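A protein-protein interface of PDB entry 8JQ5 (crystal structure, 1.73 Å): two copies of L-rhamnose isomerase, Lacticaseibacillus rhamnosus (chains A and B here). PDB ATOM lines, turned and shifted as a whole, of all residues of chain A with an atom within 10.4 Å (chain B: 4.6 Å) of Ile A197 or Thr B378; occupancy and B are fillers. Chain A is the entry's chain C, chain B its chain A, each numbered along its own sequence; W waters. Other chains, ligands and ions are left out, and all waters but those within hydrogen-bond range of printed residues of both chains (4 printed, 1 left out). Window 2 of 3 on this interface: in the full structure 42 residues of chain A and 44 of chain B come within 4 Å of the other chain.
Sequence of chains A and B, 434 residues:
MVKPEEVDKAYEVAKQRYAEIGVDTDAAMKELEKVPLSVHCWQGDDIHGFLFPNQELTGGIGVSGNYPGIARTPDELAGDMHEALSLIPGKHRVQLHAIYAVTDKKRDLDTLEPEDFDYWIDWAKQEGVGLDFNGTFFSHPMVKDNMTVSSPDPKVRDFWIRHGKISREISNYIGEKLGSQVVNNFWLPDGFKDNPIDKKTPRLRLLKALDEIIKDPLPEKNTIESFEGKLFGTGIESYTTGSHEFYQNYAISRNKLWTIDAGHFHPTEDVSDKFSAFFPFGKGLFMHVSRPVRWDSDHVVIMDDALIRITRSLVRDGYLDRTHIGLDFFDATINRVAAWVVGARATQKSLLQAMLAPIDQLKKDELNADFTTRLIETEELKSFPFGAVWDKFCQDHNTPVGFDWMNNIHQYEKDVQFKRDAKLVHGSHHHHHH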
ATOM      1  N   MET A 147      30.846 -20.087  -2.173  1.00  0.00           N
ATOM      2  CA  MET A 147      31.811 -19.619  -1.147  1.00  0.00           C
ATOM      3  C   MET A 147      31.927 -20.643  -0.013  1.00  0.00           C
ATOM      4  O   MET A 147      30.962 -21.401   0.243  1.00  0.00           O
ATOM      5  CB  MET A 147      31.422 -18.245  -0.604  1.00  0.00           C
ATOM      6  CG  MET A 147      31.443 -17.156  -1.676  1.00  0.00           C
ATOM      7  SD  MET A 147      31.086 -15.547  -0.955  1.00  0.00           S
ATOM      8  CE  MET A 147      31.195 -14.450  -2.368  1.00  0.00           C
ATOM      9  N   GLY A 191      33.882 -16.921  -4.942  1.00  0.00           N
ATOM     10  CA  GLY A 191      33.791 -15.696  -5.751  1.00  0.00           C
ATOM     11  C   GLY A 191      32.365 -15.429  -6.171  1.00  0.00           C
ATOM     12  O   GLY A 191      31.455 -15.964  -5.512  1.00  0.00           O
ATOM     13  N   PHE A 192      32.176 -14.649  -7.237  1.00  0.00           N
ATOM     14  CA  PHE A 192      30.832 -14.274  -7.742  1.00  0.00           C
ATOM     15  C   PHE A 192      30.717 -14.599  -9.227  1.00  0.00           C
ATOM     16  O   PHE A 192      31.687 -14.379  -9.983  1.00  0.00           O
ATOM     17  CB  PHE A 192      30.580 -12.779  -7.559  1.00  0.00           C
ATOM     18  CG  PHE A 192      30.352 -12.343  -6.136  1.00  0.00           C
ATOM     19  CD1 PHE A 192      29.157 -12.625  -5.495  1.00  0.00           C
ATOM     20  CD2 PHE A 192      31.313 -11.614  -5.462  1.00  0.00           C
ATOM     21  CE1 PHE A 192      28.929 -12.187  -4.206  1.00  0.00           C
ATOM     22  CE2 PHE A 192      31.085 -11.185  -4.165  1.00  0.00           C
ATOM     23  CZ  PHE A 192      29.891 -11.466  -3.544  1.00  0.00           C
ATOM     24  N   LYS A 193      29.550 -15.099  -9.618  1.00  0.00           N
ATOM     25  CA  LYS A 193      29.160 -15.227 -11.042  1.00  0.00           C
ATOM     26  C   LYS A 193      29.133 -13.848 -11.705  1.00  0.00           C
ATOM     27  O   LYS A 193      29.652 -13.727 -12.837  1.00  0.00           O
ATOM     28  CB  LYS A 193      27.799 -15.910 -11.153  1.00  0.00           C
ATOM     29  CG  LYS A 193      27.328 -16.036 -12.589  1.00  0.00           C
ATOM     30  CD  LYS A 193      26.151 -16.932 -12.797  1.00  0.00           C
ATOM     31  CE  LYS A 193      25.733 -16.918 -14.255  1.00  0.00           C
ATOM     32  NZ  LYS A 193      24.803 -18.022 -14.581  1.00  0.00           N
ATOM     33  N   ASP A 194      28.511 -12.851 -11.066  1.00  0.00           N
ATOM     34  CA  ASP A 194      28.304 -11.521 -11.703  1.00  0.00           C
ATOM     35  C   ASP A 194      29.053 -10.459 -10.892  1.00  0.00           C
ATOM     36  O   ASP A 194      29.718 -10.819  -9.903  1.00  0.00           O
ATOM     37  CB  ASP A 194      26.818 -11.197 -11.887  1.00  0.00           C
ATOM     38  CG  ASP A 194      26.503 -10.541 -13.221  1.00  0.00           C
ATOM     39  OD1 ASP A 194      27.242  -9.621 -13.614  1.00  0.00           O
ATOM     40  OD2 ASP A 194      25.519 -10.962 -13.855  1.00  0.00           O
ATOM     41  N   ASN A 195      28.993  -9.210 -11.355  1.00  0.00           N
ATOM     42  CA  ASN A 195      29.838  -8.099 -10.865  1.00  0.00           C
ATOM     43  C   ASN A 195      29.488  -7.809  -9.417  1.00  0.00           C
ATOM     44  O   ASN A 195      28.342  -7.534  -9.083  1.00  0.00           O
ATOM     45  CB  ASN A 195      29.701  -6.858 -11.738  1.00  0.00           C
ATOM     46  CG  ASN A 195      30.278  -7.098 -13.114  1.00  0.00           C
ATOM     47  OD1 ASN A 195      31.385  -7.625 -13.242  1.00  0.00           O
ATOM     48  ND2 ASN A 195      29.519  -6.756 -14.137  1.00  0.00           N
ATOM     49  N   PRO A 196      30.488  -7.895  -8.520  1.00  0.00           N
ATOM     50  CA  PRO A 196      30.278  -7.589  -7.113  1.00  0.00           C
ATOM     51  C   PRO A 196      30.306  -6.089  -6.796  1.00  0.00           C
ATOM     52  O   PRO A 196      30.946  -5.324  -7.512  1.00  0.00           O
ATOM     53  CB  PRO A 196      31.470  -8.295  -6.466  1.00  0.00           C
ATOM     54  CG  PRO A 196      32.559  -8.119  -7.478  1.00  0.00           C
ATOM     55  CD  PRO A 196      31.863  -8.343  -8.804  1.00  0.00           C
ATOM     56  N   ILE A 197      29.601  -5.717  -5.726  1.00  0.00           N
ATOM     57  CA  ILE A 197      29.619  -4.345  -5.145  1.00  0.00           C
ATOM     58  C   ILE A 197      30.843  -4.218  -4.237  1.00  0.00           C
ATOM     59  O   ILE A 197      31.545  -3.195  -4.330  1.00  0.00           O
ATOM     60  CB  ILE A 197      28.328  -4.054  -4.363  1.00  0.00           C
ATOM     61  CG1 ILE A 197      27.066  -4.326  -5.188  1.00  0.00           C
ATOM     62  CG2 ILE A 197      28.358  -2.635  -3.825  1.00  0.00           C
ATOM     63  CD1 ILE A 197      26.965  -3.504  -6.454  1.00  0.00           C
ATOM     64  N   ASP A 198      31.064  -5.216  -3.376  1.00  0.00           N
ATOM     65  CA  ASP A 198      32.124  -5.199  -2.331  1.00  0.00           C
ATOM     66  C   ASP A 198      33.200  -6.232  -2.678  1.00  0.00           C
ATOM     67  O   ASP A 198      32.933  -7.443  -2.525  1.00  0.00           O
ATOM     68  CB  ASP A 198      31.531  -5.434  -0.939  1.00  0.00           C
ATOM     69  CG  ASP A 198      32.538  -5.244   0.178  1.00  0.00           C
ATOM     70  OD1 ASP A 198      33.729  -5.461  -0.086  1.00  0.00           O
ATOM     71  OD2 ASP A 198      32.119  -4.876   1.299  1.00  0.00           O
ATOM     72  N   LYS A 199      34.367  -5.763  -3.132  1.00  0.00           N
ATOM     73  CA  LYS A 199      35.525  -6.629  -3.475  1.00  0.00           C
ATOM     74  C   LYS A 199      36.455  -6.744  -2.260  1.00  0.00           C
ATOM     75  O   LYS A 199      37.216  -7.712  -2.190  1.00  0.00           O
ATOM     76  CB  LYS A 199      36.290  -6.044  -4.660  1.00  0.00           C
ATOM     77  CG  LYS A 199      35.498  -5.920  -5.953  1.00  0.00           C
ATOM     78  CD  LYS A 199      36.324  -5.356  -7.092  1.00  0.00           C
ATOM     79  CE  LYS A 199      35.589  -5.319  -8.411  1.00  0.00           C
ATOM     80  NZ  LYS A 199      36.458  -4.819  -9.511  1.00  0.00           N
ATOM     81  N   LYS A 200      36.389  -5.778  -1.346  1.00  0.00           N
ATOM     82  CA  LYS A 200      37.314  -5.671  -0.184  1.00  0.00           C
ATOM     83  C   LYS A 200      36.976  -6.718   0.884  1.00  0.00           C
ATOM     84  O   LYS A 200      37.879  -7.457   1.311  1.00  0.00           O
ATOM     85  CB  LYS A 200      37.209  -4.269   0.416  1.00  0.00           C
ATOM     86  CG  LYS A 200      37.812  -4.147   1.805  1.00  0.00           C
ATOM     87  CD  LYS A 200      37.825  -2.743   2.340  1.00  0.00           C
ATOM     88  CE  LYS A 200      36.446  -2.231   2.682  1.00  0.00           C
ATOM     89  NZ  LYS A 200      36.526  -0.887   3.296  1.00  0.00           N
ATOM     90  N   THR A 201      35.717  -6.766   1.322  1.00  0.00           N
ATOM     91  CA  THR A 201      35.280  -7.547   2.507  1.00  0.00           C
ATOM     92  C   THR A 201      35.476  -9.047   2.265  1.00  0.00           C
ATOM     93  O   THR A 201      35.963  -9.739   3.145  1.00  0.00           O
ATOM     94  CB  THR A 201      33.864  -7.143   2.932  1.00  0.00           C
ATOM     95  OG1 THR A 201      33.881  -5.727   3.116  1.00  0.00           O
ATOM     96  CG2 THR A 201      33.417  -7.824   4.206  1.00  0.00           C
ATOM     97  N   PRO A 202      35.123  -9.635   1.096  1.00  0.00           N
ATOM     98  CA  PRO A 202      35.397 -11.054   0.874  1.00  0.00           C
ATOM     99  C   PRO A 202      36.878 -11.389   1.119  1.00  0.00           C
ATOM    100  O   PRO A 202      37.162 -12.400   1.722  1.00  0.00           O
ATOM    101  CB  PRO A 202      34.993 -11.273  -0.590  1.00  0.00           C
ATOM    102  CG  PRO A 202      33.939 -10.217  -0.831  1.00  0.00           C
ATOM    103  CD  PRO A 202      34.411  -9.019  -0.032  1.00  0.00           C
ATOM    104  N   ARG A 205      37.720 -11.311   4.792  1.00  0.00           N
ATOM    105  CA  ARG A 205      37.171 -12.563   5.393  1.00  0.00           C
ATOM    106  C   ARG A 205      38.131 -13.720   5.071  1.00  0.00           C
ATOM    107  O   ARG A 205      38.412 -14.562   5.967  1.00  0.00           O
ATOM    108  CB  ARG A 205      35.749 -12.832   4.880  1.00  0.00           C
ATOM    109  CG  ARG A 205      34.687 -11.898   5.440  1.00  0.00           C
ATOM    110  CD  ARG A 205      33.279 -12.425   5.218  1.00  0.00           C
ATOM    111  NE  ARG A 205      33.034 -12.828   3.844  1.00  0.00           N
ATOM    112  CZ  ARG A 205      32.378 -12.104   2.931  1.00  0.00           C
ATOM    113  NH1 ARG A 205      31.888 -10.916   3.240  1.00  0.00           N
ATOM    114  NH2 ARG A 205      32.223 -12.571   1.703  1.00  0.00           N
ATOM    115  N   SER A 238      32.991 -13.662 -12.722  1.00  0.00           N
ATOM    116  CA  SER A 238      33.168 -12.184 -12.621  1.00  0.00           C
ATOM    117  C   SER A 238      34.154 -11.801 -11.508  1.00  0.00           C
ATOM    118  O   SER A 238      34.819 -10.756 -11.627  1.00  0.00           O
ATOM    119  CB  SER A 238      31.836 -11.484 -12.443  1.00  0.00           C
ATOM    120  OG  SER A 238      31.043 -11.584 -13.622  1.00  0.00           O
ATOM    121  N   TYR A 239      34.264 -12.593 -10.449  1.00  0.00           N
ATOM    122  CA  TYR A 239      35.129 -12.247  -9.293  1.00  0.00           C
ATOM    123  C   TYR A 239      35.571 -13.527  -8.602  1.00  0.00           C
ATOM    124  O   TYR A 239      34.734 -14.412  -8.369  1.00  0.00           O
ATOM    125  CB  TYR A 239      34.381 -11.326  -8.328  1.00  0.00           C
ATOM    126  CG  TYR A 239      35.073 -11.027  -7.023  1.00  0.00           C
ATOM    127  CD1 TYR A 239      34.887 -11.838  -5.914  1.00  0.00           C
ATOM    128  CD2 TYR A 239      35.864  -9.904  -6.871  1.00  0.00           C
ATOM    129  CE1 TYR A 239      35.464 -11.545  -4.696  1.00  0.00           C
ATOM    130  CE2 TYR A 239      36.454  -9.598  -5.657  1.00  0.00           C
ATOM    131  CZ  TYR A 239      36.256 -10.421  -4.564  1.00  0.00           C
ATOM    132  OH  TYR A 239      36.842 -10.137  -3.364  1.00  0.00           O
ATOM    133  N   ARG B 316      33.351   2.283  -3.992  1.00  0.00           N
ATOM    134  CA  ARG B 316      32.526   1.275  -3.266  1.00  0.00           C
ATOM    135  C   ARG B 316      33.319   0.716  -2.084  1.00  0.00           C
ATOM    136  O   ARG B 316      32.720   0.449  -1.045  1.00  0.00           O
ATOM    137  CB  ARG B 316      32.089   0.147  -4.204  1.00  0.00           C
ATOM    138  CG  ARG B 316      31.073   0.576  -5.255  1.00  0.00           C
ATOM    139  CD  ARG B 316      30.924  -0.472  -6.339  1.00  0.00           C
ATOM    140  NE  ARG B 316      29.768  -0.239  -7.187  1.00  0.00           N
ATOM    141  CZ  ARG B 316      29.404  -1.025  -8.191  1.00  0.00           C
ATOM    142  NH1 ARG B 316      30.100  -2.115  -8.477  1.00  0.00           N
ATOM    143  NH2 ARG B 316      28.329  -0.728  -8.893  1.00  0.00           N
ATOM    144  N   ASP B 317      34.624   0.527  -2.231  1.00  0.00           N
ATOM    145  CA  ASP B 317      35.420  -0.151  -1.173  1.00  0.00           C
ATOM    146  C   ASP B 317      36.177   0.885  -0.333  1.00  0.00           C
ATOM    147  O   ASP B 317      37.007   0.464   0.494  1.00  0.00           O
ATOM    148  CB  ASP B 317      36.299  -1.250  -1.775  1.00  0.00           C
ATOM    149  CG  ASP B 317      35.496  -2.455  -2.257  1.00  0.00           C
ATOM    150  OD1 ASP B 317      34.491  -2.807  -1.592  1.00  0.00           O
ATOM    151  OD2 ASP B 317      35.876  -3.033  -3.283  1.00  0.00           O
ATOM    152  N   ILE B 359      25.056   2.457  -1.937  1.00  0.00           N
ATOM    153  CA  ILE B 359      26.140   1.446  -1.820  1.00  0.00           C
ATOM    154  C   ILE B 359      25.898   0.589  -0.573  1.00  0.00           C
ATOM    155  O   ILE B 359      26.009  -0.651  -0.688  1.00  0.00           O
ATOM    156  CB  ILE B 359      27.523   2.118  -1.849  1.00  0.00           C
ATOM    157  CG1 ILE B 359      27.808   2.727  -3.226  1.00  0.00           C
ATOM    158  CG2 ILE B 359      28.600   1.126  -1.449  1.00  0.00           C
ATOM    159  CD1 ILE B 359      28.971   3.686  -3.242  1.00  0.00           C
ATOM    160  N   LEU B 362      23.097  -1.846  -1.328  1.00  0.00           N
ATOM    161  CA  LEU B 362      23.534  -2.814  -2.369  1.00  0.00           C
ATOM    162  C   LEU B 362      24.466  -3.859  -1.730  1.00  0.00           C
ATOM    163  O   LEU B 362      24.345  -5.059  -2.062  1.00  0.00           O
ATOM    164  CB  LEU B 362      24.206  -2.048  -3.511  1.00  0.00           C
ATOM    165  CG  LEU B 362      23.242  -1.473  -4.541  1.00  0.00           C
ATOM    166  CD1 LEU B 362      23.955  -0.507  -5.469  1.00  0.00           C
ATOM    167  CD2 LEU B 362      22.583  -2.590  -5.327  1.00  0.00           C
ATOM    168  N   LYS B 363      25.335  -3.437  -0.813  1.00  0.00           N
ATOM    169  CA  LYS B 363      26.242  -4.354  -0.077  1.00  0.00           C
ATOM    170  C   LYS B 363      25.419  -5.334   0.768  1.00  0.00           C
ATOM    171  O   LYS B 363      25.754  -6.526   0.743  1.00  0.00           O
ATOM    172  CB  LYS B 363      27.233  -3.564   0.779  1.00  0.00           C
ATOM    173  CG  LYS B 363      28.328  -2.859  -0.009  1.00  0.00           C
ATOM    174  CD  LYS B 363      29.304  -2.138   0.882  1.00  0.00           C
ATOM    175  CE  LYS B 363      30.452  -1.512   0.125  1.00  0.00           C
ATOM    176  NZ  LYS B 363      31.466  -0.960   1.054  1.00  0.00           N
ATOM    177  N   GLU B 366      23.744  -7.858  -1.458  1.00  0.00           N
ATOM    178  CA  GLU B 366      24.800  -8.781  -1.945  1.00  0.00           C
ATOM    179  C   GLU B 366      25.167  -9.772  -0.831  1.00  0.00           C
ATOM    180  O   GLU B 366      25.273 -10.977  -1.123  1.00  0.00           O
ATOM    181  CB  GLU B 366      25.996  -7.958  -2.413  1.00  0.00           C
ATOM    182  CG  GLU B 366      27.219  -8.779  -2.743  1.00  0.00           C
ATOM    183  CD  GLU B 366      28.259  -7.950  -3.472  1.00  0.00           C
ATOM    184  OE1 GLU B 366      29.156  -7.401  -2.800  1.00  0.00           O
ATOM    185  OE2 GLU B 366      28.133  -7.815  -4.709  1.00  0.00           O
ATOM    186  N   ARG B 374      20.667  -6.884  -7.130  1.00  0.00           N
ATOM    187  CA  ARG B 374      21.961  -6.232  -7.453  1.00  0.00           C
ATOM    188  C   ARG B 374      22.023  -5.946  -8.956  1.00  0.00           C
ATOM    189  O   ARG B 374      22.400  -4.815  -9.335  1.00  0.00           O
ATOM    190  CB  ARG B 374      23.150  -7.097  -7.043  1.00  0.00           C
ATOM    191  CG  ARG B 374      24.489  -6.386  -7.181  1.00  0.00           C
ATOM    192  CD  ARG B 374      25.639  -7.329  -6.888  1.00  0.00           C
ATOM    193  NE  ARG B 374      25.571  -8.476  -7.784  1.00  0.00           N
ATOM    194  CZ  ARG B 374      26.172  -9.635  -7.571  1.00  0.00           C
ATOM    195  NH1 ARG B 374      26.907  -9.810  -6.488  1.00  0.00           N
ATOM    196  NH2 ARG B 374      26.051 -10.613  -8.449  1.00  0.00           N
ATOM    197  N   LEU B 375      21.677  -6.926  -9.789  1.00  0.00           N
ATOM    198  CA  LEU B 375      21.764  -6.778 -11.270  1.00  0.00           C
ATOM    199  C   LEU B 375      20.780  -5.703 -11.743  1.00  0.00           C
ATOM    200  O   LEU B 375      21.196  -4.823 -12.523  1.00  0.00           O
ATOM    201  CB  LEU B 375      21.486  -8.114 -11.961  1.00  0.00           C
ATOM    202  CG  LEU B 375      21.580  -8.072 -13.489  1.00  0.00           C
ATOM    203  CD1 LEU B 375      23.003  -7.788 -13.939  1.00  0.00           C
ATOM    204  CD2 LEU B 375      21.063  -9.364 -14.110  1.00  0.00           C
ATOM    205  N   ILE B 376      19.514  -5.789 -11.328  1.00  0.00           N
ATOM    206  CA  ILE B 376      18.466  -4.815 -11.748  1.00  0.00           C
ATOM    207  C   ILE B 376      18.931  -3.402 -11.386  1.00  0.00           C
ATOM    208  O   ILE B 376      18.934  -2.527 -12.277  1.00  0.00           O
ATOM    209  CB  ILE B 376      17.117  -5.140 -11.095  1.00  0.00           C
ATOM    210  CG1 ILE B 376      16.619  -6.518 -11.529  1.00  0.00           C
ATOM    211  CG2 ILE B 376      16.117  -4.026 -11.392  1.00  0.00           C
ATOM    212  CD1 ILE B 376      15.337  -6.953 -10.861  1.00  0.00           C
ATOM    213  N   GLU B 377      19.322  -3.183 -10.134  1.00  0.00           N
ATOM    214  CA  GLU B 377      19.617  -1.815  -9.623  1.00  0.00           C
ATOM    215  C   GLU B 377      20.879  -1.262 -10.296  1.00  0.00           C
ATOM    216  O   GLU B 377      20.844  -0.113 -10.722  1.00  0.00           O
ATOM    217  CB  GLU B 377      19.725  -1.803  -8.099  1.00  0.00           C
ATOM    218  CG  GLU B 377      18.386  -1.983  -7.409  1.00  0.00           C
ATOM    219  CD  GLU B 377      18.415  -1.742  -5.910  1.00  0.00           C
ATOM    220  OE1 GLU B 377      19.458  -1.255  -5.411  1.00  0.00           O
ATOM    221  OE2 GLU B 377      17.399  -2.039  -5.245  1.00  0.00           O
ATOM    222  N   THR B 378      21.976  -2.026 -10.367  1.00  0.00           N
ATOM    223  CA  THR B 378      23.224  -1.528 -11.000  1.00  0.00           C
ATOM    224  C   THR B 378      22.938  -1.140 -12.450  1.00  0.00           C
ATOM    225  O   THR B 378      23.481  -0.118 -12.899  1.00  0.00           O
ATOM    226  CB  THR B 378      24.380  -2.519 -10.844  1.00  0.00           C
ATOM    227  OG1 THR B 378      23.996  -3.807 -11.330  1.00  0.00           O
ATOM    228  CG2 THR B 378      24.814  -2.603  -9.399  1.00  0.00           C
ATOM    229  N   GLU B 379      22.108  -1.909 -13.151  1.00  0.00           N
ATOM    230  CA  GLU B 379      21.752  -1.621 -14.564  1.00  0.00           C
ATOM    231  C   GLU B 379      20.865  -0.368 -14.627  1.00  0.00           C
ATOM    232  O   GLU B 379      21.140   0.501 -15.471  1.00  0.00           O
ATOM    233  CB  GLU B 379      21.149  -2.871 -15.199  1.00  0.00           C
ATOM    234  CG  GLU B 379      22.207  -3.880 -15.597  1.00  0.00           C
ATOM    235  CD  GLU B 379      23.394  -3.257 -16.311  1.00  0.00           C
ATOM    236  OE1 GLU B 379      23.166  -2.672 -17.402  1.00  0.00           O
ATOM    237  OE2 GLU B 379      24.540  -3.331 -15.760  1.00  0.00           O
ATOM    238  N   GLU B 380      19.863  -0.241 -13.754  1.00  0.00           N
ATOM    239  CA  GLU B 380      18.982   0.954 -13.742  1.00  0.00           C
ATOM    240  C   GLU B 380      19.823   2.206 -13.477  1.00  0.00           C
ATOM    241  O   GLU B 380      19.571   3.235 -14.122  1.00  0.00           O
ATOM    242  CB  GLU B 380      17.859   0.797 -12.720  1.00  0.00           C
ATOM    243  CG  GLU B 380      16.812  -0.218 -13.125  1.00  0.00           C
ATOM    244  CD  GLU B 380      16.220  -0.010 -14.506  1.00  0.00           C
ATOM    245  OE1 GLU B 380      16.066   1.161 -14.907  1.00  0.00           O
ATOM    246  OE2 GLU B 380      15.930  -1.023 -15.184  1.00  0.00           O
ATOM    247  N   LEU B 381      20.803   2.124 -12.574  1.00  0.00           N
ATOM    248  CA  LEU B 381      21.616   3.301 -12.174  1.00  0.00           C
ATOM    249  C   LEU B 381      22.406   3.833 -13.378  1.00  0.00           C
ATOM    250  O   LEU B 381      22.670   5.036 -13.417  1.00  0.00           O
ATOM    251  CB  LEU B 381      22.520   2.918 -11.001  1.00  0.00           C
ATOM    252  CG  LEU B 381      21.784   2.792  -9.668  1.00  0.00           C
ATOM    253  CD1 LEU B 381      22.666   2.158  -8.616  1.00  0.00           C
ATOM    254  CD2 LEU B 381      21.270   4.144  -9.199  1.00  0.00           C
ATOM    255  N   LYS B 382      22.727   2.994 -14.361  1.00  0.00           N
ATOM    256  CA  LYS B 382      23.479   3.446 -15.554  1.00  0.00           C
ATOM    257  C   LYS B 382      22.640   4.441 -16.362  1.00  0.00           C
ATOM    258  O   LYS B 382      23.248   5.180 -17.155  1.00  0.00           O
ATOM    259  CB  LYS B 382      23.909   2.253 -16.410  1.00  0.00           C
ATOM    260  CG  LYS B 382      24.902   1.348 -15.708  1.00  0.00           C
ATOM    261  CD  LYS B 382      25.321   0.165 -16.529  1.00  0.00           C
ATOM    262  CE  LYS B 382      26.471  -0.581 -15.895  1.00  0.00           C
ATOM    263  NZ  LYS B 382      26.714  -1.872 -16.578  1.00  0.00           N
HETATM  264  O   HOH W   1      30.896  -8.989  -1.339  1.00  0.00           O
HETATM  265  O   HOH W   2      34.015  -2.528  -5.381  1.00  0.00           O
HETATM  266  O   HOH W   3      32.792  -3.051  -7.771  1.00  0.00           O
HETATM  267  O   HOH W   4      33.670  -2.382   0.833  1.00  0.00           O
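The guanidinium group (NE) of Arg B374 is in hydrogen-bond range of the backbone carbonyl oxygen (O) of Asn A195 (3.2 Å). OE1 of Glu B366 lies within hydrogen-bond range of N of Asp A198. OD2 of Asp A198 lies within salt-bridge range of NZ of Lys B363, at 3.98 Å. The guanidinium group (NH1) of Arg B316 sits at hydrogen-bond distance from the backbone carbonyl oxygen (O) of Pro A196 (3.5 Å). OD1 of Asp B317 lies close to OD1 of Asp A198, at 3.1 Å. OD2 of Asp B317 sits at hydrogen-bond distance from N of Lys A199 (3.1 Å). The backbone carbonyl oxygen of Asp B317 sits at hydrogen-bond distance from the side-chain amino group of Lys A200 (3.1 Å). OE2 of Glu B366 is in hydrogen-bond range of N of Ile A197, at 2.8 Å.
The backbone carbonyl oxygen (O) of Leu B375 sits at hydrogen-bond distance from the side-chain hydroxyl (OG1) of Thr B378, at 3.2 Å. OG1 of Thr B378 lies within hydrogen-bond range of O of Arg B374, at 2.7 Å. The backbone carbonyl oxygen (O) of Arg B316 lies within hydrogen-bond range of the side-chain amino group (NZ) of Lys B363 (2.8 Å). The backbone NH of Phe A192 lies within hydrogen-bond range of the backbone carbonyl oxygen of Tyr A239. N of Ser A238 lies within hydrogen-bond range of O of Phe A192, 3.1 Å away. OD1 of Asp A198 is in hydrogen-bond range of N of Lys A200, at 3.0 Å.
Among the printed residues, merely in contact across the chains: Phe A192 with Glu B366 (3.9 Å), Phe A192 with Arg B374 (3.7 Å), Asp A194 with Arg B374 (3.6 Å), Pro A196 with Glu B366 (3.2 Å), Ile A197 with Arg B316 (3.4 Å), Ile A197 with Lys B363 (3.8 Å), Ile A197 with Arg B374 (3.7 Å) and Ile A197 with Thr B378 (3.8 Å).
Ile A197 touches just these residues of chain B: Arg B316, Lys B363, Glu B366, Arg B374 and Thr B378. Thr B378 touches just one residue of chain A: Ile A197. No residue of chain A comes within 4 Å of Leu B362. Lys B363 touches just these residues of chain A: Ile A197 (3.8 Å) and Asp A198 (3.9 Å). No residue of chain A comes within 4 Å of Glu B379. No residue of chain A comes within 4 Å of Leu B381. Of the printed residues of chain B, Asp A198 touches Asp B317, Lys B363 and Glu B366. Of the printed residues of chain B, Pro A196 touches Arg B316 (3.5 Å) and Glu B366 (3.2 Å). Of the printed residues of chain B, Lys A200 touches Asp B317. Pro A202 touches none of the printed residues of chain B. Ser A238 touches none of the printed residues of chain B.
Of the 16 printed residues of chain A, 8 touch a printed residue of chain B. Printed residues of chain A that touch a printed residue of chain B: Phe A192, Asp A194, Asn A195, Pro A196, Ile A197, Asp A198, Lys A199 and Lys A200. Hydrophobic or aromatic side chains of chain A within 4 Å of the printed part of chain B: Phe A192, Pro A196 and Ile A197. Of the 15 printed residues of chain B, 6 touch a printed residue of chain A. Along chain B the printed residues that touch a printed residue of chain A span positions 316 to 378. Among the printed residues, 16 pairs touch across the chains. Among the printed residues, Asp or Glu carboxylates within 4 Å of a Lys or Arg side-chain nitrogen of the other chain: Asp A198 with Lys B363 (3.98 Å).
No position is printed for both chains. Of the 16 pairs that touch across the chains among the printed residues, none has its exchanged pair printed and touching as well.
Water W4 lies within hydrogen-bond range of the side-chain carboxylate (OD1) of Asp B317 (2.6 Å), the side-chain amino group (NZ) of Lys B363 (2.6 Å) and the side-chain carboxylate (OD2) of Asp A198 (3.0 Å). Water W2 bridges the backbone carbonyl oxygen (O) of Ile A197 and the side-chain carboxylate (OD2) of Asp B317. Water W1 bridges OE1 of Glu B366 (2.8 Å) and O of Asp A198 (2.8 Å). Water W3 bridges the guanidinium group of Arg B316 and the backbone carbonyl oxygen of Pro A196.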
